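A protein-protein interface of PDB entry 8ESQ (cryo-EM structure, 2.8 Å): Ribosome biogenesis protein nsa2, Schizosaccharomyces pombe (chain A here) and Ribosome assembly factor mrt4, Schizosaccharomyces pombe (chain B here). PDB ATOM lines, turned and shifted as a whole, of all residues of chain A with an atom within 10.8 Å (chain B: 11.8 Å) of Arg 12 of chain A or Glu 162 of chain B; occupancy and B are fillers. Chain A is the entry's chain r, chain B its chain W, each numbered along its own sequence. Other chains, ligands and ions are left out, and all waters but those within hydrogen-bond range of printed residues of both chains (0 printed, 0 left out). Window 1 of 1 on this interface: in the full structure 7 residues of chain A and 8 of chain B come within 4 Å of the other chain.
The backbone NH (N) of Asn 176 of chain B lies close to the backbone carbonyl oxygen (O) of Lys 13 of chain A (3.3 Å).
The backbone NH (N) of Gly 177 of chain B lies within hydrogen-bond range of the backbone carbonyl oxygen (O) of Lys 13 of chain A, at 2.6 Å.
O of Leu 174 of chain B lies close to O of His 14 of chain A, 2.8 Å away.
The backbone carbonyl oxygen (O) of Ser 10 of chain A sits at hydrogen-bond distance from a ring nitrogen (ND1) of His 14 of chain A (3.1 Å).
Among the printed residues, pairs that only touch across the chains: Arg 12 of chain A with Glu 162 of chain B, Arg 12 of chain A with Gly 177 of chain B and Glu 21 of chain A with Arg 166 of chain B.
Ile 7 of chain A touches none of the printed residues of chain B.
Ser 10 of chain A touches none of the printed residues of chain B.
No residue of chain B comes within 4 Å of Ile 11 of chain A.
Printed residues of chain B within 4 Å of His 14 of chain A: Leu 174.
Of the printed residues of chain B, Glu 21 of chain A touches Arg 166 (3.5 Å).
No residue of chain A comes within 4 Å of Thr 160 of chain B.
Of chain A, only Arg 12 (3.3 Å) comes within 4 Å of Glu 162 of chain B.
No residue of chain A comes within 4 Å of Pro 163 of chain B.
No residue of chain A comes within 4 Å of Gln 164 of chain B.
No residue of chain A comes within 4 Å of Val 165 of chain B.
Of the printed residues of chain A, Arg 166 of chain B touches Glu 21 (3.5 Å).
Of the printed residues of chain A, Leu 174 of chain B touches His 14.
Of the printed residues of chain A, Asn 176 of chain B touches Lys 13 (3.2 Å).
The nearest residue of chain B that does not touch Arg 12 of chain A is Pro 163 of chain B (4.7 Å).
The nearest printed residue of chain A that does not touch Leu 174 of chain B is Lys 13 of chain A (4.4 Å).
Hydrophobic or aromatic side chains of chain B within 4 Å of the printed part of chain A: Leu 174.
Among the printed residues, no Asp or Glu carboxylate lies within 4 Å of a Lys or Arg side-chain nitrogen of the other chain.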
ATOM      1  N   GLU A   5      -5.748  -6.977  19.557  1.00  0.00           N
ATOM      2  CA  GLU A   5      -4.828  -7.260  18.455  1.00  0.00           C
ATOM      3  C   GLU A   5      -3.616  -6.331  18.548  1.00  0.00           C
ATOM      4  O   GLU A   5      -3.501  -5.328  17.843  1.00  0.00           O
ATOM      5  CB  GLU A   5      -5.553  -7.093  17.126  1.00  0.00           C
ATOM      6  CG  GLU A   5      -6.642  -8.123  16.874  1.00  0.00           C
ATOM      7  CD  GLU A   5      -7.032  -8.204  15.413  1.00  0.00           C
ATOM      8  OE1 GLU A   5      -6.977  -7.162  14.727  1.00  0.00           O
ATOM      9  OE2 GLU A   5      -7.396  -9.306  14.949  1.00  0.00           O
ATOM     10  N   TYR A   6      -2.688  -6.691  19.440  1.00  0.00           N
ATOM     11  CA  TYR A   6      -1.614  -5.754  19.758  1.00  0.00           C
ATOM     12  C   TYR A   6      -0.455  -5.859  18.772  1.00  0.00           C
ATOM     13  O   TYR A   6       0.268  -4.879  18.558  1.00  0.00           O
ATOM     14  CB  TYR A   6      -1.130  -5.938  21.199  1.00  0.00           C
ATOM     15  CG  TYR A   6      -0.997  -7.356  21.702  1.00  0.00           C
ATOM     16  CD1 TYR A   6      -2.098  -8.057  22.176  1.00  0.00           C
ATOM     17  CD2 TYR A   6       0.238  -7.991  21.718  1.00  0.00           C
ATOM     18  CE1 TYR A   6      -1.977  -9.351  22.642  1.00  0.00           C
ATOM     19  CE2 TYR A   6       0.371  -9.284  22.189  1.00  0.00           C
ATOM     20  CZ  TYR A   6      -0.741  -9.960  22.647  1.00  0.00           C
ATOM     21  OH  TYR A   6      -0.616 -11.248  23.113  1.00  0.00           O
ATOM     22  N   ILE A   7      -0.245  -7.029  18.164  1.00  0.00           N
ATOM     23  CA  ILE A   7       0.743  -7.088  17.089  1.00  0.00           C
ATOM     24  C   ILE A   7       0.228  -6.343  15.866  1.00  0.00           C
ATOM     25  O   ILE A   7       0.986  -5.640  15.189  1.00  0.00           O
ATOM     26  CB  ILE A   7       1.144  -8.542  16.758  1.00  0.00           C
ATOM     27  CG1 ILE A   7      -0.021  -9.334  16.165  1.00  0.00           C
ATOM     28  CG2 ILE A   7       1.751  -9.232  17.976  1.00  0.00           C
ATOM     29  CD1 ILE A   7       0.371 -10.712  15.673  1.00  0.00           C
ATOM     30  N   GLU A   8      -1.075  -6.456  15.585  1.00  0.00           N
ATOM     31  CA  GLU A   8      -1.657  -5.723  14.466  1.00  0.00           C
ATOM     32  C   GLU A   8      -1.471  -4.223  14.636  1.00  0.00           C
ATOM     33  O   GLU A   8      -1.130  -3.520  13.678  1.00  0.00           O
ATOM     34  CB  GLU A   8      -3.141  -6.060  14.327  1.00  0.00           C
ATOM     35  CG  GLU A   8      -3.434  -7.526  14.095  1.00  0.00           C
ATOM     36  CD  GLU A   8      -2.846  -8.034  12.795  1.00  0.00           C
ATOM     37  OE1 GLU A   8      -2.786  -7.251  11.824  1.00  0.00           O
ATOM     38  OE2 GLU A   8      -2.451  -9.217  12.741  1.00  0.00           O
ATOM     39  N   GLU A   9      -1.683  -3.715  15.851  1.00  0.00           N
ATOM     40  CA  GLU A   9      -1.462  -2.295  16.101  1.00  0.00           C
ATOM     41  C   GLU A   9      -0.006  -1.920  15.867  1.00  0.00           C
ATOM     42  O   GLU A   9       0.286  -0.877  15.271  1.00  0.00           O
ATOM     43  CB  GLU A   9      -1.892  -1.940  17.523  1.00  0.00           C
ATOM     44  CG  GLU A   9      -3.385  -2.060  17.753  1.00  0.00           C
ATOM     45  CD  GLU A   9      -3.786  -1.724  19.174  1.00  0.00           C
ATOM     46  OE1 GLU A   9      -2.887  -1.556  20.025  1.00  0.00           O
ATOM     47  OE2 GLU A   9      -5.002  -1.628  19.439  1.00  0.00           O
ATOM     48  N   SER A  10       0.924  -2.761  16.323  1.00  0.00           N
ATOM     49  CA  SER A  10       2.336  -2.497  16.067  1.00  0.00           C
ATOM     50  C   SER A  10       2.668  -2.663  14.589  1.00  0.00           C
ATOM     51  O   SER A  10       3.475  -1.904  14.042  1.00  0.00           O
ATOM     52  CB  SER A  10       3.212  -3.404  16.929  1.00  0.00           C
ATOM     53  OG  SER A  10       2.568  -4.630  17.200  1.00  0.00           O
ATOM     54  N   ILE A  11       2.061  -3.650  13.924  1.00  0.00           N
ATOM     55  CA  ILE A  11       2.211  -3.749  12.474  1.00  0.00           C
ATOM     56  C   ILE A  11       1.657  -2.501  11.803  1.00  0.00           C
ATOM     57  O   ILE A  11       2.258  -1.961  10.866  1.00  0.00           O
ATOM     58  CB  ILE A  11       1.536  -5.027  11.940  1.00  0.00           C
ATOM     59  CG1 ILE A  11       2.223  -6.274  12.500  1.00  0.00           C
ATOM     60  CG2 ILE A  11       1.561  -5.050  10.421  1.00  0.00           C
ATOM     61  CD1 ILE A  11       1.397  -7.534  12.370  1.00  0.00           C
ATOM     62  N   ARG A  12       0.503  -2.020  12.269  1.00  0.00           N
ATOM     63  CA  ARG A  12      -0.036  -0.772  11.741  1.00  0.00           C
ATOM     64  C   ARG A  12       0.885   0.403  12.048  1.00  0.00           C
ATOM     65  O   ARG A  12       1.094   1.275  11.197  1.00  0.00           O
ATOM     66  CB  ARG A  12      -1.435  -0.516  12.305  1.00  0.00           C
ATOM     67  CG  ARG A  12      -2.508  -1.470  11.797  1.00  0.00           C
ATOM     68  CD  ARG A  12      -2.860  -1.207  10.344  1.00  0.00           C
ATOM     69  NE  ARG A  12      -2.059  -2.022   9.439  1.00  0.00           N
ATOM     70  CZ  ARG A  12      -1.940  -1.802   8.137  1.00  0.00           C
ATOM     71  NH1 ARG A  12      -2.567  -0.799   7.545  1.00  0.00           N
ATOM     72  NH2 ARG A  12      -1.172  -2.610   7.411  1.00  0.00           N
ATOM     73  N   LYS A  13       1.448   0.442  13.256  1.00  0.00           N
ATOM     74  CA  LYS A  13       2.204   1.601  13.712  1.00  0.00           C
ATOM     75  C   LYS A  13       3.709   1.478  13.489  1.00  0.00           C
ATOM     76  O   LYS A  13       4.403   2.500  13.508  1.00  0.00           O
ATOM     77  CB  LYS A  13       1.927   1.853  15.199  1.00  0.00           C
ATOM     78  CG  LYS A  13       2.238   3.265  15.669  1.00  0.00           C
ATOM     79  CD  LYS A  13       1.425   4.292  14.896  1.00  0.00           C
ATOM     80  CE  LYS A  13      -0.060   4.167  15.201  1.00  0.00           C
ATOM     81  NZ  LYS A  13      -0.865   5.196  14.485  1.00  0.00           N
ATOM     82  N   HIS A  14       4.231   0.278  13.279  1.00  0.00           N
ATOM     83  CA  HIS A  14       5.665   0.131  13.039  1.00  0.00           C
ATOM     84  C   HIS A  14       5.977  -0.585  11.735  1.00  0.00           C
ATOM     85  O   HIS A  14       6.975  -0.259  11.089  1.00  0.00           O
ATOM     86  CB  HIS A  14       6.331  -0.615  14.207  1.00  0.00           C
ATOM     87  CG  HIS A  14       5.970  -0.073  15.554  1.00  0.00           C
ATOM     88  ND1 HIS A  14       5.116  -0.728  16.414  1.00  0.00           N
ATOM     89  CD2 HIS A  14       6.350   1.059  16.190  1.00  0.00           C
ATOM     90  CE1 HIS A  14       4.981  -0.021  17.521  1.00  0.00           C
ATOM     91  NE2 HIS A  14       5.721   1.069  17.412  1.00  0.00           N
ATOM     92  N   GLY A  15       5.159  -1.546  11.335  1.00  0.00           N
ATOM     93  CA  GLY A  15       5.302  -2.207  10.056  1.00  0.00           C
ATOM     94  C   GLY A  15       5.601  -3.687  10.198  1.00  0.00           C
ATOM     95  O   GLY A  15       5.857  -4.205  11.284  1.00  0.00           O
ATOM     96  N   ARG A  16       5.553  -4.361   9.055  1.00  0.00           N
ATOM     97  CA  ARG A  16       5.857  -5.776   8.934  1.00  0.00           C
ATOM     98  C   ARG A  16       7.361  -5.946   8.714  1.00  0.00           C
ATOM     99  O   ARG A  16       8.082  -4.985   8.439  1.00  0.00           O
ATOM    100  CB  ARG A  16       5.038  -6.380   7.786  1.00  0.00           C
ATOM    101  CG  ARG A  16       5.138  -7.887   7.603  1.00  0.00           C
ATOM    102  CD  ARG A  16       4.724  -8.618   8.867  1.00  0.00           C
ATOM    103  NE  ARG A  16       5.856  -9.273   9.509  1.00  0.00           N
ATOM    104  CZ  ARG A  16       5.821  -9.818  10.716  1.00  0.00           C
ATOM    105  NH1 ARG A  16       4.720  -9.800  11.450  1.00  0.00           N
ATOM    106  NH2 ARG A  16       6.916 -10.399  11.199  1.00  0.00           N
ATOM    107  N   ARG A  17       7.838  -7.182   8.852  1.00  0.00           N
ATOM    108  CA  ARG A  17       9.263  -7.448   8.712  1.00  0.00           C
ATOM    109  C   ARG A  17       9.747  -7.052   7.320  1.00  0.00           C
ATOM    110  O   ARG A  17       9.029  -7.188   6.325  1.00  0.00           O
ATOM    111  CB  ARG A  17       9.560  -8.920   8.986  1.00  0.00           C
ATOM    112  CG  ARG A  17      11.035  -9.228   9.122  1.00  0.00           C
ATOM    113  CD  ARG A  17      11.256 -10.683   9.471  1.00  0.00           C
ATOM    114  NE  ARG A  17      12.672 -11.021   9.531  1.00  0.00           N
ATOM    115  CZ  ARG A  17      13.452 -10.798  10.580  1.00  0.00           C
ATOM    116  NH1 ARG A  17      12.988 -10.225  11.679  1.00  0.00           N
ATOM    117  NH2 ARG A  17      14.731 -11.158  10.525  1.00  0.00           N
ATOM    118  N   GLU A  21       7.886 -10.385   3.066  1.00  0.00           N
ATOM    119  CA  GLU A  21       7.190 -10.663   1.813  1.00  0.00           C
ATOM    120  C   GLU A  21       8.038 -11.524   0.885  1.00  0.00           C
ATOM    121  O   GLU A  21       7.552 -12.508   0.317  1.00  0.00           O
ATOM    122  CB  GLU A  21       6.801  -9.353   1.130  1.00  0.00           C
ATOM    123  CG  GLU A  21       5.655  -8.620   1.807  1.00  0.00           C
ATOM    124  CD  GLU A  21       5.112  -7.482   0.965  1.00  0.00           C
ATOM    125  OE1 GLU A  21       5.689  -7.208  -0.108  1.00  0.00           O
ATOM    126  OE2 GLU A  21       4.107  -6.865   1.374  1.00  0.00           O
ATOM    127  N   VAL B 142       5.772  11.025   2.420  1.00  0.00           N
ATOM    128  CA  VAL B 142       5.504  11.039   0.988  1.00  0.00           C
ATOM    129  C   VAL B 142       4.199  11.774   0.708  1.00  0.00           C
ATOM    130  O   VAL B 142       3.305  11.857   1.561  1.00  0.00           O
ATOM    131  CB  VAL B 142       5.466   9.606   0.427  1.00  0.00           C
ATOM    132  N   SER B 144       0.993  12.153  -2.161  1.00  0.00           N
ATOM    133  CA  SER B 144       0.330  11.451  -3.253  1.00  0.00           C
ATOM    134  C   SER B 144       0.210  12.308  -4.505  1.00  0.00           C
ATOM    135  O   SER B 144       0.320  11.786  -5.620  1.00  0.00           O
ATOM    136  CB  SER B 144      -1.054  10.978  -2.808  1.00  0.00           C
ATOM    137  N   LEU B 157      -2.509  14.284   1.497  1.00  0.00           N
ATOM    138  CA  LEU B 157      -1.937  12.943   1.477  1.00  0.00           C
ATOM    139  C   LEU B 157      -2.365  12.148   2.706  1.00  0.00           C
ATOM    140  O   LEU B 157      -1.928  12.430   3.821  1.00  0.00           O
ATOM    141  CB  LEU B 157      -0.411  13.011   1.398  1.00  0.00           C
ATOM    142  N   THR B 158      -3.226  11.156   2.491  1.00  0.00           N
ATOM    143  CA  THR B 158      -3.698  10.327   3.590  1.00  0.00           C
ATOM    144  C   THR B 158      -2.565   9.473   4.145  1.00  0.00           C
ATOM    145  O   THR B 158      -1.684   9.021   3.407  1.00  0.00           O
ATOM    146  CB  THR B 158      -4.849   9.433   3.127  1.00  0.00           C
ATOM    147  N   HIS B 159      -2.590   9.255   5.457  1.00  0.00           N
ATOM    148  CA  HIS B 159      -1.592   8.445   6.141  1.00  0.00           C
ATOM    149  C   HIS B 159      -2.010   6.986   6.278  1.00  0.00           C
ATOM    150  O   HIS B 159      -1.301   6.209   6.925  1.00  0.00           O
ATOM    151  CB  HIS B 159      -1.294   9.032   7.524  1.00  0.00           C
ATOM    152  N   THR B 160      -3.138   6.599   5.687  1.00  0.00           N
ATOM    153  CA  THR B 160      -3.649   5.238   5.788  1.00  0.00           C
ATOM    154  C   THR B 160      -3.039   4.293   4.761  1.00  0.00           C
ATOM    155  O   THR B 160      -3.392   3.110   4.746  1.00  0.00           O
ATOM    156  CB  THR B 160      -5.174   5.234   5.641  1.00  0.00           C
ATOM    157  N   LEU B 161      -2.139   4.780   3.908  1.00  0.00           N
ATOM    158  CA  LEU B 161      -1.511   3.931   2.903  1.00  0.00           C
ATOM    159  C   LEU B 161      -0.336   3.163   3.494  1.00  0.00           C
ATOM    160  O   LEU B 161       0.776   3.212   2.960  1.00  0.00           O
ATOM    161  CB  LEU B 161      -1.053   4.769   1.707  1.00  0.00           C
ATOM    162  N   GLU B 162      -0.574   2.458   4.600  1.00  0.00           N
ATOM    163  CA  GLU B 162       0.481   1.651   5.211  1.00  0.00           C
ATOM    164  C   GLU B 162       0.981   0.557   4.281  1.00  0.00           C
ATOM    165  O   GLU B 162       2.206   0.360   4.195  1.00  0.00           O
ATOM    166  CB  GLU B 162      -0.021   1.067   6.535  1.00  0.00           C
ATOM    167  N   PRO B 163       0.122  -0.187   3.578  1.00  0.00           N
ATOM    168  CA  PRO B 163       0.631  -1.249   2.694  1.00  0.00           C
ATOM    169  C   PRO B 163       1.524  -0.737   1.579  1.00  0.00           C
ATOM    170  O   PRO B 163       2.336  -1.506   1.048  1.00  0.00           O
ATOM    171  CB  PRO B 163      -0.653  -1.885   2.144  1.00  0.00           C
ATOM    172  N   GLN B 164       1.396   0.537   1.201  1.00  0.00           N
ATOM    173  CA  GLN B 164       2.235   1.082   0.139  1.00  0.00           C
ATOM    174  C   GLN B 164       3.708   1.090   0.529  1.00  0.00           C
ATOM    175  O   GLN B 164       4.579   1.107  -0.349  1.00  0.00           O
ATOM    176  CB  GLN B 164       1.774   2.495  -0.221  1.00  0.00           C
ATOM    177  N   VAL B 165       4.008   1.089   1.830  1.00  0.00           N
ATOM    178  CA  VAL B 165       5.399   1.073   2.274  1.00  0.00           C
ATOM    179  C   VAL B 165       6.085  -0.210   1.824  1.00  0.00           C
ATOM    180  O   VAL B 165       7.217  -0.192   1.325  1.00  0.00           O
ATOM    181  CB  VAL B 165       5.478   1.248   3.801  1.00  0.00           C
ATOM    182  N   ARG B 166       5.409  -1.346   1.995  1.00  0.00           N
ATOM    183  CA  ARG B 166       5.957  -2.620   1.549  1.00  0.00           C
ATOM    184  C   ARG B 166       5.755  -2.856   0.058  1.00  0.00           C
ATOM    185  O   ARG B 166       6.534  -3.599  -0.549  1.00  0.00           O
ATOM    186  CB  ARG B 166       5.329  -3.769   2.340  1.00  0.00           C
ATOM    187  N   GLN B 167       4.737  -2.242  -0.543  1.00  0.00           N
ATOM    188  CA  GLN B 167       4.426  -2.456  -1.950  1.00  0.00           C
ATOM    189  C   GLN B 167       5.230  -1.567  -2.887  1.00  0.00           C
ATOM    190  O   GLN B 167       5.147  -1.749  -4.107  1.00  0.00           O
ATOM    191  CB  GLN B 167       2.931  -2.232  -2.198  1.00  0.00           C
ATOM    192  N   LEU B 168       5.999  -0.616  -2.359  1.00  0.00           N
ATOM    193  CA  LEU B 168       6.777   0.285  -3.199  1.00  0.00           C
ATOM    194  C   LEU B 168       8.185  -0.243  -3.454  1.00  0.00           C
ATOM    195  O   LEU B 168       8.638  -0.282  -4.602  1.00  0.00           O
ATOM    196  CB  LEU B 168       6.844   1.675  -2.558  1.00  0.00           C
ATOM    197  N   GLY B 169       8.885  -0.652  -2.398  1.00  0.00           N
ATOM    198  CA  GLY B 169      10.254  -1.100  -2.508  1.00  0.00           C
ATOM    199  C   GLY B 169      11.291  -0.003  -2.415  1.00  0.00           C
ATOM    200  O   GLY B 169      12.490  -0.309  -2.358  1.00  0.00           O
ATOM    201  N   MET B 170      10.874   1.258  -2.397  1.00  0.00           N
ATOM    202  CA  MET B 170      11.792   2.371  -2.235  1.00  0.00           C
ATOM    203  C   MET B 170      12.248   2.476  -0.784  1.00  0.00           C
ATOM    204  O   MET B 170      11.635   1.896   0.115  1.00  0.00           O
ATOM    205  CB  MET B 170      11.126   3.672  -2.673  1.00  0.00           C
ATOM    206  N   PRO B 171      13.331   3.211  -0.528  1.00  0.00           N
ATOM    207  CA  PRO B 171      13.819   3.334   0.852  1.00  0.00           C
ATOM    208  C   PRO B 171      12.886   4.162   1.718  1.00  0.00           C
ATOM    209  O   PRO B 171      13.196   5.305   2.067  1.00  0.00           O
ATOM    210  CB  PRO B 171      15.182   4.015   0.682  1.00  0.00           C
ATOM    211  N   THR B 172      11.736   3.590   2.073  1.00  0.00           N
ATOM    212  CA  THR B 172      10.721   4.268   2.872  1.00  0.00           C
ATOM    213  C   THR B 172      10.556   3.513   4.185  1.00  0.00           C
ATOM    214  O   THR B 172      10.010   2.405   4.205  1.00  0.00           O
ATOM    215  CB  THR B 172       9.393   4.351   2.121  1.00  0.00           C
ATOM    216  N   VAL B 173      11.026   4.112   5.275  1.00  0.00           N
ATOM    217  CA  VAL B 173      10.895   3.509   6.596  1.00  0.00           C
ATOM    218  C   VAL B 173       9.527   3.853   7.166  1.00  0.00           C
ATOM    219  O   VAL B 173       9.118   5.020   7.173  1.00  0.00           O
ATOM    220  CB  VAL B 173      12.022   3.987   7.526  1.00  0.00           C
ATOM    221  N   LEU B 174       8.813   2.836   7.646  1.00  0.00           N
ATOM    222  CA  LEU B 174       7.476   3.017   8.210  1.00  0.00           C
ATOM    223  C   LEU B 174       7.623   3.346   9.690  1.00  0.00           C
ATOM    224  O   LEU B 174       7.608   2.465  10.551  1.00  0.00           O
ATOM    225  CB  LEU B 174       6.622   1.775   7.990  1.00  0.00           C
ATOM    226  N   LYS B 175       7.766   4.633   9.989  1.00  0.00           N
ATOM    227  CA  LYS B 175       7.925   5.110  11.357  1.00  0.00           C
ATOM    228  C   LYS B 175       6.612   5.703  11.848  1.00  0.00           C
ATOM    229  O   LYS B 175       6.033   6.573  11.188  1.00  0.00           O
ATOM    230  CB  LYS B 175       9.042   6.152  11.444  1.00  0.00           C
ATOM    231  N   ASN B 176       6.150   5.228  13.007  1.00  0.00           N
ATOM    232  CA  ASN B 176       4.907   5.698  13.624  1.00  0.00           C
ATOM    233  C   ASN B 176       3.721   5.543  12.674  1.00  0.00           C
ATOM    234  O   ASN B 176       2.842   6.405  12.603  1.00  0.00           O
ATOM    235  CB  ASN B 176       5.039   7.147  14.099  1.00  0.00           C
ATOM    236  N   GLY B 177       3.692   4.433  11.942  1.00  0.00           N
ATOM    237  CA  GLY B 177       2.597   4.170  11.029  1.00  0.00           C
ATOM    238  C   GLY B 177       2.522   5.095   9.837  1.00  0.00           C
ATOM    239  O   GLY B 177       1.470   5.184   9.201  1.00  0.00           O
ATOM    240  N   VAL B 178       3.610   5.790   9.514  1.00  0.00           N
ATOM    241  CA  VAL B 178       3.656   6.718   8.391  1.00  0.00           C
ATOM    242  C   VAL B 178       4.918   6.439   7.590  1.00  0.00           C
ATOM    243  O   VAL B 178       6.003   6.292   8.164  1.00  0.00           O
ATOM    244  CB  VAL B 178       3.625   8.185   8.857  1.00  0.00           C
ATOM    245  N   VAL B 179       4.776   6.364   6.267  1.00  0.00           N
ATOM    246  CA  VAL B 179       5.927   6.134   5.403  1.00  0.00           C
ATOM    247  C   VAL B 179       6.828   7.360   5.428  1.00  0.00           C
ATOM    248  O   VAL B 179       6.372   8.492   5.217  1.00  0.00           O
ATOM    249  CB  VAL B 179       5.472   5.806   3.973  1.00  0.00           C
ATOM    250  N   THR B 180       8.114   7.142   5.688  1.00  0.00           N
ATOM    251  CA  THR B 180       9.096   8.215   5.751  1.00  0.00           C
ATOM    252  C   THR B 180      10.250   7.889   4.816  1.00  0.00           C
ATOM    253  O   THR B 180      10.816   6.794   4.883  1.00  0.00           O
ATOM    254  CB  THR B 180       9.615   8.414   7.179  1.00  0.00           C
